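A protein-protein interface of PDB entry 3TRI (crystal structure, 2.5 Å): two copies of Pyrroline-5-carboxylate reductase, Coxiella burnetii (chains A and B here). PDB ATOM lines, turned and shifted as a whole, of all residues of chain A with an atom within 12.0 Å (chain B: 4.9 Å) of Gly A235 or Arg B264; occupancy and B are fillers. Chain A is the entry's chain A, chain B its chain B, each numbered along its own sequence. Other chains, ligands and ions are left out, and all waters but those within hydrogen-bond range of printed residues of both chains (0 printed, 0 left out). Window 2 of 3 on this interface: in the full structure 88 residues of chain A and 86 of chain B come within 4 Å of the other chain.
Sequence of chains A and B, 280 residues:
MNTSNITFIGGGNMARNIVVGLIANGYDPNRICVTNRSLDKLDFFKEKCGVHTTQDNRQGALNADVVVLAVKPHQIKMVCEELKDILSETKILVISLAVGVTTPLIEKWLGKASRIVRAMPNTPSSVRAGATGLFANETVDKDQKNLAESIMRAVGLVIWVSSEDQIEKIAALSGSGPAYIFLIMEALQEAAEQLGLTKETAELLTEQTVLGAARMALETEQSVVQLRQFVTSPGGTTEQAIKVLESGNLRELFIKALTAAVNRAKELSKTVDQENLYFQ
No position is printed for both chains.
Of the 11 pairs that touch across the chains among the printed residues, none has its exchanged pair printed and touching as well.
The backbone NH of Gly A235 sits at hydrogen-bond distance from the side-chain carboxylate of Glu A239 (2.7 Å).
NZ of Lys A243 sits close to NE2 of Gln A240.
O of Thr B259 sits close to ND2 of Asn B263 (3.1 Å).
NH1 of Arg B264 is in salt-bridge range of OE1 of Glu B267 (3.5 Å).
Leu A195 touches Thr B259.
Leu A195 touches Val B262.
CG of Arg B264 touches O of Gly A236, 3.8 Å away.
Thr A237 touches Ala B261.
Arg B264 touches Thr A237 (CG to N, 3.8 Å).
OG1 of Thr A237 touches CA of Ala B265 (3.7 Å).
Gln A240 touches Ala B260 (CB to O, 3.8 Å).
Arg B264 touches Gln A240 (CB to CG, 3.6 Å).
Ala A241 touches Ala B261 (CB to CB, 3.9 Å).
Val A244 touches Ala B260.
Printed residues of chain B within 4 Å of Gly A235: Arg B264 (2.7 Å).
Of the printed residues of chain A, Arg B264 touches Gly A235 (2.7 Å), Gly A236 (3.8 Å), Thr A237 (3.8 Å) and Gln A240 (3.6 Å).
Of chain A, only Leu A195 (3.4 Å) comes within 4 Å of Val B262.
No residue of chain A comes within 4 Å of Asn B263.
Ala B265 touches just one residue of chain A: Thr A237.
No residue of chain A comes within 4 Å of Lys B266.
No residue of chain A comes within 4 Å of Leu B268.
Printed residues of chain B within 4 Å of Gln A240: Ala B260 and Arg B264.
Of the printed residues of chain B, Ala A241 touches Ala B261.
Of the printed residues of chain B, Thr A237 touches Ala B261, Arg B264 and Ala B265.
Printed residues of chain B within 4 Å of Gly A236: Arg B264.
Gln A229 touches none of the printed residues of chain B.
The nearest residue of chain B that does not touch Gly A235 is Leu B268 (4.3 Å).
The nearest printed residue of chain B that does not touch Leu A195 is Ala B260 (6.5 Å).
Of the 10 printed residues of chain B, 6 touch a printed residue of chain A.
Printed residues of chain A that touch a printed residue of chain B: Leu A195, Gly A235, Gly A236, Thr A237, Gln A240, Ala A241 and Val A244.
Hydrophobic or aromatic side chains of chain A that line the printed part of chain B: Leu A195, Ala A241 and Val A244.
Among the printed residues, 11 pairs touch across the chains.
Among the printed residues, no Asp or Glu carboxylate lies within 4 Å of a Lys or Arg side-chain nitrogen of the other chain.
The backbone carbonyl oxygen (O) of Gly A235 lies within hydrogen-bond range of the guanidinium group (NE) of Arg B264, 2.7 Å away.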
ATOM      1  N   LEU A 195     -14.225  12.586  17.923  1.00  0.00           N
ATOM      2  CA  LEU A 195     -13.688  11.944  16.724  1.00  0.00           C
ATOM      3  C   LEU A 195     -14.483  10.707  16.327  1.00  0.00           C
ATOM      4  O   LEU A 195     -14.296  10.175  15.233  1.00  0.00           O
ATOM      5  CB  LEU A 195     -12.215  11.559  16.897  1.00  0.00           C
ATOM      6  CG  LEU A 195     -11.196  12.637  17.269  1.00  0.00           C
ATOM      7  CD1 LEU A 195      -9.843  12.247  16.710  1.00  0.00           C
ATOM      8  CD2 LEU A 195     -11.603  14.011  16.767  1.00  0.00           C
ATOM      9  N   ARG A 228       9.004  12.383  26.216  1.00  0.00           N
ATOM     10  CA  ARG A 228       8.178  12.947  25.152  1.00  0.00           C
ATOM     11  C   ARG A 228       8.906  12.868  23.816  1.00  0.00           C
ATOM     12  O   ARG A 228       8.337  12.436  22.816  1.00  0.00           O
ATOM     13  CB  ARG A 228       7.798  14.394  25.461  1.00  0.00           C
ATOM     14  CG  ARG A 228       6.755  14.978  24.520  1.00  0.00           C
ATOM     15  CD  ARG A 228       6.233  16.318  25.024  1.00  0.00           C
ATOM     16  NE  ARG A 228       6.673  17.428  24.181  1.00  0.00           N
ATOM     17  CZ  ARG A 228       7.387  18.464  24.610  1.00  0.00           C
ATOM     18  NH1 ARG A 228       7.746  18.552  25.883  1.00  0.00           N
ATOM     19  NH2 ARG A 228       7.736  19.421  23.762  1.00  0.00           N
ATOM     20  N   GLN A 229      10.169  13.285  23.808  1.00  0.00           N
ATOM     21  CA  GLN A 229      11.009  13.179  22.618  1.00  0.00           C
ATOM     22  C   GLN A 229      11.103  11.733  22.138  1.00  0.00           C
ATOM     23  O   GLN A 229      10.845  11.437  20.971  1.00  0.00           O
ATOM     24  CB  GLN A 229      12.410  13.729  22.900  1.00  0.00           C
ATOM     25  CG  GLN A 229      12.439  15.223  23.185  1.00  0.00           C
ATOM     26  CD  GLN A 229      13.662  15.649  23.984  1.00  0.00           C
ATOM     27  OE1 GLN A 229      14.606  14.876  24.159  1.00  0.00           O
ATOM     28  NE2 GLN A 229      13.642  16.883  24.480  1.00  0.00           N
ATOM     29  N   PHE A 230      11.466  10.837  23.050  1.00  0.00           N
ATOM     30  CA  PHE A 230      11.592   9.421  22.731  1.00  0.00           C
ATOM     31  C   PHE A 230      10.323   8.869  22.077  1.00  0.00           C
ATOM     32  O   PHE A 230      10.380   7.942  21.269  1.00  0.00           O
ATOM     33  CB  PHE A 230      11.934   8.622  23.993  1.00  0.00           C
ATOM     34  CG  PHE A 230      11.788   7.137  23.823  1.00  0.00           C
ATOM     35  CD1 PHE A 230      12.769   6.399  23.184  1.00  0.00           C
ATOM     36  CD2 PHE A 230      10.665   6.480  24.297  1.00  0.00           C
ATOM     37  CE1 PHE A 230      12.634   5.031  23.022  1.00  0.00           C
ATOM     38  CE2 PHE A 230      10.524   5.114  24.139  1.00  0.00           C
ATOM     39  CZ  PHE A 230      11.510   4.390  23.502  1.00  0.00           C
ATOM     40  N   VAL A 231       9.185   9.451  22.423  1.00  0.00           N
ATOM     41  CA  VAL A 231       7.895   8.954  21.965  1.00  0.00           C
ATOM     42  C   VAL A 231       7.407   9.653  20.687  1.00  0.00           C
ATOM     43  O   VAL A 231       6.497   9.175  20.010  1.00  0.00           O
ATOM     44  CB  VAL A 231       6.845   9.086  23.098  1.00  0.00           C
ATOM     45  CG1 VAL A 231       5.556   9.706  22.590  1.00  0.00           C
ATOM     46  CG2 VAL A 231       6.599   7.727  23.763  1.00  0.00           C
ATOM     47  N   THR A 232       8.031  10.773  20.348  1.00  0.00           N
ATOM     48  CA  THR A 232       7.607  11.559  19.198  1.00  0.00           C
ATOM     49  C   THR A 232       8.559  11.395  18.015  1.00  0.00           C
ATOM     50  O   THR A 232       9.704  11.829  18.068  1.00  0.00           O
ATOM     51  CB  THR A 232       7.519  13.059  19.547  1.00  0.00           C
ATOM     52  OG1 THR A 232       6.650  13.244  20.671  1.00  0.00           O
ATOM     53  CG2 THR A 232       6.998  13.858  18.359  1.00  0.00           C
ATOM     54  N   SER A 233       8.081  10.765  16.949  1.00  0.00           N
ATOM     55  CA  SER A 233       8.845  10.685  15.715  1.00  0.00           C
ATOM     56  C   SER A 233       8.496  11.874  14.825  1.00  0.00           C
ATOM     57  O   SER A 233       7.372  12.372  14.861  1.00  0.00           O
ATOM     58  CB  SER A 233       8.575   9.364  14.991  1.00  0.00           C
ATOM     59  OG  SER A 233       7.189   9.072  14.949  1.00  0.00           O
ATOM     60  N   PRO A 234       9.470  12.343  14.033  1.00  0.00           N
ATOM     61  CA  PRO A 234       9.261  13.509  13.170  1.00  0.00           C
ATOM     62  C   PRO A 234       8.263  13.224  12.049  1.00  0.00           C
ATOM     63  O   PRO A 234       8.256  12.136  11.474  1.00  0.00           O
ATOM     64  CB  PRO A 234      10.659  13.772  12.590  1.00  0.00           C
ATOM     65  CG  PRO A 234      11.604  13.063  13.519  1.00  0.00           C
ATOM     66  CD  PRO A 234      10.855  11.853  13.966  1.00  0.00           C
ATOM     67  N   GLY A 235       7.420  14.208  11.754  1.00  0.00           N
ATOM     68  CA  GLY A 235       6.422  14.081  10.711  1.00  0.00           C
ATOM     69  C   GLY A 235       5.290  13.133  11.052  1.00  0.00           C
ATOM     70  O   GLY A 235       4.353  12.979  10.273  1.00  0.00           O
ATOM     71  N   GLY A 236       5.368  12.508  12.222  1.00  0.00           N
ATOM     72  CA  GLY A 236       4.412  11.484  12.607  1.00  0.00           C
ATOM     73  C   GLY A 236       3.092  11.967  13.187  1.00  0.00           C
ATOM     74  O   GLY A 236       2.872  13.163  13.387  1.00  0.00           O
ATOM     75  N   THR A 237       2.210  11.010  13.452  1.00  0.00           N
ATOM     76  CA  THR A 237       0.913  11.264  14.066  1.00  0.00           C
ATOM     77  C   THR A 237       1.030  12.087  15.346  1.00  0.00           C
ATOM     78  O   THR A 237       0.389  13.133  15.486  1.00  0.00           O
ATOM     79  CB  THR A 237       0.211   9.933  14.390  1.00  0.00           C
ATOM     80  OG1 THR A 237      -0.055   9.228  13.172  1.00  0.00           O
ATOM     81  CG2 THR A 237      -1.091  10.170  15.126  1.00  0.00           C
ATOM     82  N   THR A 238       1.856  11.610  16.272  1.00  0.00           N
ATOM     83  CA  THR A 238       2.017  12.242  17.579  1.00  0.00           C
ATOM     84  C   THR A 238       2.500  13.687  17.483  1.00  0.00           C
ATOM     85  O   THR A 238       1.994  14.568  18.179  1.00  0.00           O
ATOM     86  CB  THR A 238       2.999  11.450  18.465  1.00  0.00           C
ATOM     87  OG1 THR A 238       2.603  10.074  18.517  1.00  0.00           O
ATOM     88  CG2 THR A 238       3.019  12.018  19.866  1.00  0.00           C
ATOM     89  N   GLU A 239       3.485  13.926  16.627  1.00  0.00           N
ATOM     90  CA  GLU A 239       4.039  15.264  16.461  1.00  0.00           C
ATOM     91  C   GLU A 239       2.976  16.280  16.034  1.00  0.00           C
ATOM     92  O   GLU A 239       2.925  17.398  16.548  1.00  0.00           O
ATOM     93  CB  GLU A 239       5.172  15.236  15.444  1.00  0.00           C
ATOM     94  CG  GLU A 239       5.875  16.557  15.269  1.00  0.00           C
ATOM     95  CD  GLU A 239       6.843  16.525  14.108  1.00  0.00           C
ATOM     96  OE1 GLU A 239       6.381  16.397  12.953  1.00  0.00           O
ATOM     97  OE2 GLU A 239       8.062  16.613  14.352  1.00  0.00           O
ATOM     98  N   GLN A 240       2.125  15.891  15.095  1.00  0.00           N
ATOM     99  CA  GLN A 240       1.027  16.760  14.691  1.00  0.00           C
ATOM    100  C   GLN A 240       0.211  17.213  15.900  1.00  0.00           C
ATOM    101  O   GLN A 240      -0.029  18.407  16.085  1.00  0.00           O
ATOM    102  CB  GLN A 240       0.126  16.063  13.667  1.00  0.00           C
ATOM    103  CG  GLN A 240       0.816  15.812  12.345  1.00  0.00           C
ATOM    104  CD  GLN A 240       1.583  17.029  11.873  1.00  0.00           C
ATOM    105  OE1 GLN A 240       0.992  18.066  11.561  1.00  0.00           O
ATOM    106  NE2 GLN A 240       2.909  16.915  11.832  1.00  0.00           N
ATOM    107  N   ALA A 241      -0.203  16.254  16.722  1.00  0.00           N
ATOM    108  CA  ALA A 241      -1.027  16.543  17.890  1.00  0.00           C
ATOM    109  C   ALA A 241      -0.281  17.424  18.888  1.00  0.00           C
ATOM    110  O   ALA A 241      -0.842  18.374  19.435  1.00  0.00           O
ATOM    111  CB  ALA A 241      -1.492  15.252  18.551  1.00  0.00           C
ATOM    112  N   ILE A 242       0.990  17.109  19.111  1.00  0.00           N
ATOM    113  CA  ILE A 242       1.822  17.893  20.017  1.00  0.00           C
ATOM    114  C   ILE A 242       1.903  19.354  19.583  1.00  0.00           C
ATOM    115  O   ILE A 242       1.749  20.260  20.401  1.00  0.00           O
ATOM    116  CB  ILE A 242       3.242  17.307  20.126  1.00  0.00           C
ATOM    117  CG1 ILE A 242       3.186  15.899  20.717  1.00  0.00           C
ATOM    118  CG2 ILE A 242       4.127  18.205  20.979  1.00  0.00           C
ATOM    119  CD1 ILE A 242       2.585  15.852  22.100  1.00  0.00           C
ATOM    120  N   LYS A 243       2.139  19.581  18.296  1.00  0.00           N
ATOM    121  CA  LYS A 243       2.212  20.941  17.773  1.00  0.00           C
ATOM    122  C   LYS A 243       0.932  21.726  18.043  1.00  0.00           C
ATOM    123  O   LYS A 243       0.982  22.910  18.360  1.00  0.00           O
ATOM    124  CB  LYS A 243       2.565  20.941  16.282  1.00  0.00           C
ATOM    125  CG  LYS A 243       4.020  20.571  16.011  1.00  0.00           C
ATOM    126  CD  LYS A 243       4.413  20.796  14.560  1.00  0.00           C
ATOM    127  CE  LYS A 243       3.765  19.775  13.640  1.00  0.00           C
ATOM    128  NZ  LYS A 243       4.266  19.896  12.241  1.00  0.00           N
ATOM    129  N   VAL A 244      -0.216  21.064  17.936  1.00  0.00           N
ATOM    130  CA  VAL A 244      -1.472  21.698  18.320  1.00  0.00           C
ATOM    131  C   VAL A 244      -1.461  22.040  19.807  1.00  0.00           C
ATOM    132  O   VAL A 244      -1.810  23.150  20.203  1.00  0.00           O
ATOM    133  CB  VAL A 244      -2.681  20.797  18.039  1.00  0.00           C
ATOM    134  CG1 VAL A 244      -3.963  21.494  18.464  1.00  0.00           C
ATOM    135  CG2 VAL A 244      -2.734  20.420  16.566  1.00  0.00           C
ATOM    136  N   THR B 259      -7.522  15.529  16.053  1.00  0.00           N
ATOM    137  CA  THR B 259      -7.882  15.667  14.651  1.00  0.00           C
ATOM    138  C   THR B 259      -6.627  15.741  13.785  1.00  0.00           C
ATOM    139  O   THR B 259      -6.513  15.038  12.780  1.00  0.00           O
ATOM    140  CB  THR B 259      -8.767  16.902  14.411  1.00  0.00           C
ATOM    141  OG1 THR B 259     -10.050  16.689  15.014  1.00  0.00           O
ATOM    142  CG2 THR B 259      -8.952  17.141  12.916  1.00  0.00           C
ATOM    143  N   ALA B 260      -5.683  16.588  14.184  1.00  0.00           N
ATOM    144  CA  ALA B 260      -4.404  16.677  13.494  1.00  0.00           C
ATOM    145  C   ALA B 260      -3.750  15.301  13.435  1.00  0.00           C
ATOM    146  O   ALA B 260      -3.260  14.877  12.385  1.00  0.00           O
ATOM    147  CB  ALA B 260      -3.489  17.668  14.196  1.00  0.00           C
ATOM    148  N   ALA B 261      -3.760  14.606  14.568  1.00  0.00           N
ATOM    149  CA  ALA B 261      -3.170  13.273  14.664  1.00  0.00           C
ATOM    150  C   ALA B 261      -3.842  12.270  13.728  1.00  0.00           C
ATOM    151  O   ALA B 261      -3.166  11.562  12.982  1.00  0.00           O
ATOM    152  CB  ALA B 261      -3.215  12.778  16.105  1.00  0.00           C
ATOM    153  N   VAL B 262      -5.170  12.212  13.768  1.00  0.00           N
ATOM    154  CA  VAL B 262      -5.917  11.283  12.926  1.00  0.00           C
ATOM    155  C   VAL B 262      -5.733  11.594  11.440  1.00  0.00           C
ATOM    156  O   VAL B 262      -5.575  10.686  10.626  1.00  0.00           O
ATOM    157  CB  VAL B 262      -7.425  11.281  13.265  1.00  0.00           C
ATOM    158  CG1 VAL B 262      -8.206  10.481  12.230  1.00  0.00           C
ATOM    159  CG2 VAL B 262      -7.653  10.710  14.644  1.00  0.00           C
ATOM    160  N   ASN B 263      -5.767  12.876  11.089  1.00  0.00           N
ATOM    161  CA  ASN B 263      -5.534  13.275   9.711  1.00  0.00           C
ATOM    162  C   ASN B 263      -4.186  12.764   9.227  1.00  0.00           C
ATOM    163  O   ASN B 263      -4.077  12.217   8.133  1.00  0.00           O
ATOM    164  CB  ASN B 263      -5.610  14.795   9.561  1.00  0.00           C
ATOM    165  CG  ASN B 263      -7.015  15.330   9.748  1.00  0.00           C
ATOM    166  OD1 ASN B 263      -7.993  14.626   9.510  1.00  0.00           O
ATOM    167  ND2 ASN B 263      -7.121  16.584  10.177  1.00  0.00           N
ATOM    168  N   ARG B 264      -3.166  12.936  10.057  1.00  0.00           N
ATOM    169  CA  ARG B 264      -1.833  12.462   9.728  1.00  0.00           C
ATOM    170  C   ARG B 264      -1.809  10.936   9.634  1.00  0.00           C
ATOM    171  O   ARG B 264      -1.141  10.366   8.770  1.00  0.00           O
ATOM    172  CB  ARG B 264      -0.817  12.958  10.763  1.00  0.00           C
ATOM    173  CG  ARG B 264       0.640  12.711  10.379  1.00  0.00           C
ATOM    174  CD  ARG B 264       0.904  13.174   8.958  1.00  0.00           C
ATOM    175  NE  ARG B 264       2.299  13.002   8.566  1.00  0.00           N
ATOM    176  CZ  ARG B 264       2.695  12.673   7.338  1.00  0.00           C
ATOM    177  NH1 ARG B 264       1.796  12.466   6.383  1.00  0.00           N
ATOM    178  NH2 ARG B 264       3.991  12.540   7.068  1.00  0.00           N
ATOM    179  N   ALA B 265      -2.547  10.278  10.521  1.00  0.00           N
ATOM    180  CA  ALA B 265      -2.594   8.820  10.529  1.00  0.00           C
ATOM    181  C   ALA B 265      -3.186   8.292   9.229  1.00  0.00           C
ATOM    182  O   ALA B 265      -2.685   7.320   8.665  1.00  0.00           O
ATOM    183  CB  ALA B 265      -3.389   8.320  11.718  1.00  0.00           C
ATOM    184  N   LYS B 266      -4.251   8.938   8.758  1.00  0.00           N
ATOM    185  CA  LYS B 266      -4.877   8.569   7.492  1.00  0.00           C
ATOM    186  C   LYS B 266      -3.908   8.718   6.322  1.00  0.00           C
ATOM    187  O   LYS B 266      -3.773   7.809   5.504  1.00  0.00           O
ATOM    188  CB  LYS B 266      -6.130   9.410   7.231  1.00  0.00           C
ATOM    189  CG  LYS B 266      -7.262   9.195   8.224  1.00  0.00           C
ATOM    190  CD  LYS B 266      -8.616   9.452   7.577  1.00  0.00           C
ATOM    191  CE  LYS B 266      -9.525  10.289   8.469  1.00  0.00           C
ATOM    192  NZ  LYS B 266      -9.077  11.713   8.557  1.00  0.00           N
ATOM    193  N   GLU B 267      -3.243   9.868   6.245  1.00  0.00           N
ATOM    194  CA  GLU B 267      -2.249  10.107   5.202  1.00  0.00           C
ATOM    195  C   GLU B 267      -1.158   9.039   5.213  1.00  0.00           C
ATOM    196  O   GLU B 267      -0.695   8.599   4.162  1.00  0.00           O
ATOM    197  CB  GLU B 267      -1.607  11.483   5.376  1.00  0.00           C
ATOM    198  CG  GLU B 267      -2.565  12.651   5.277  1.00  0.00           C
ATOM    199  CD  GLU B 267      -1.884  13.978   5.564  1.00  0.00           C
ATOM    200  OE1 GLU B 267      -1.241  14.100   6.628  1.00  0.00           O
ATOM    201  OE2 GLU B 267      -1.982  14.895   4.722  1.00  0.00           O
ATOM    202  N   LEU B 268      -0.748   8.629   6.410  1.00  0.00           N
ATOM    203  CA  LEU B 268       0.344   7.673   6.568  1.00  0.00           C
ATOM    204  C   LEU B 268      -0.145   6.241   6.450  1.00  0.00           C
ATOM    205  O   LEU B 268       0.650   5.301   6.464  1.00  0.00           O
ATOM    206  CB  LEU B 268       1.025   7.863   7.923  1.00  0.00           C
ATOM    207  CG  LEU B 268       1.674   9.223   8.177  1.00  0.00           C
ATOM    208  CD1 LEU B 268       2.159   9.320   9.614  1.00  0.00           C
ATOM    209  CD2 LEU B 268       2.811   9.466   7.193  1.00  0.00           C
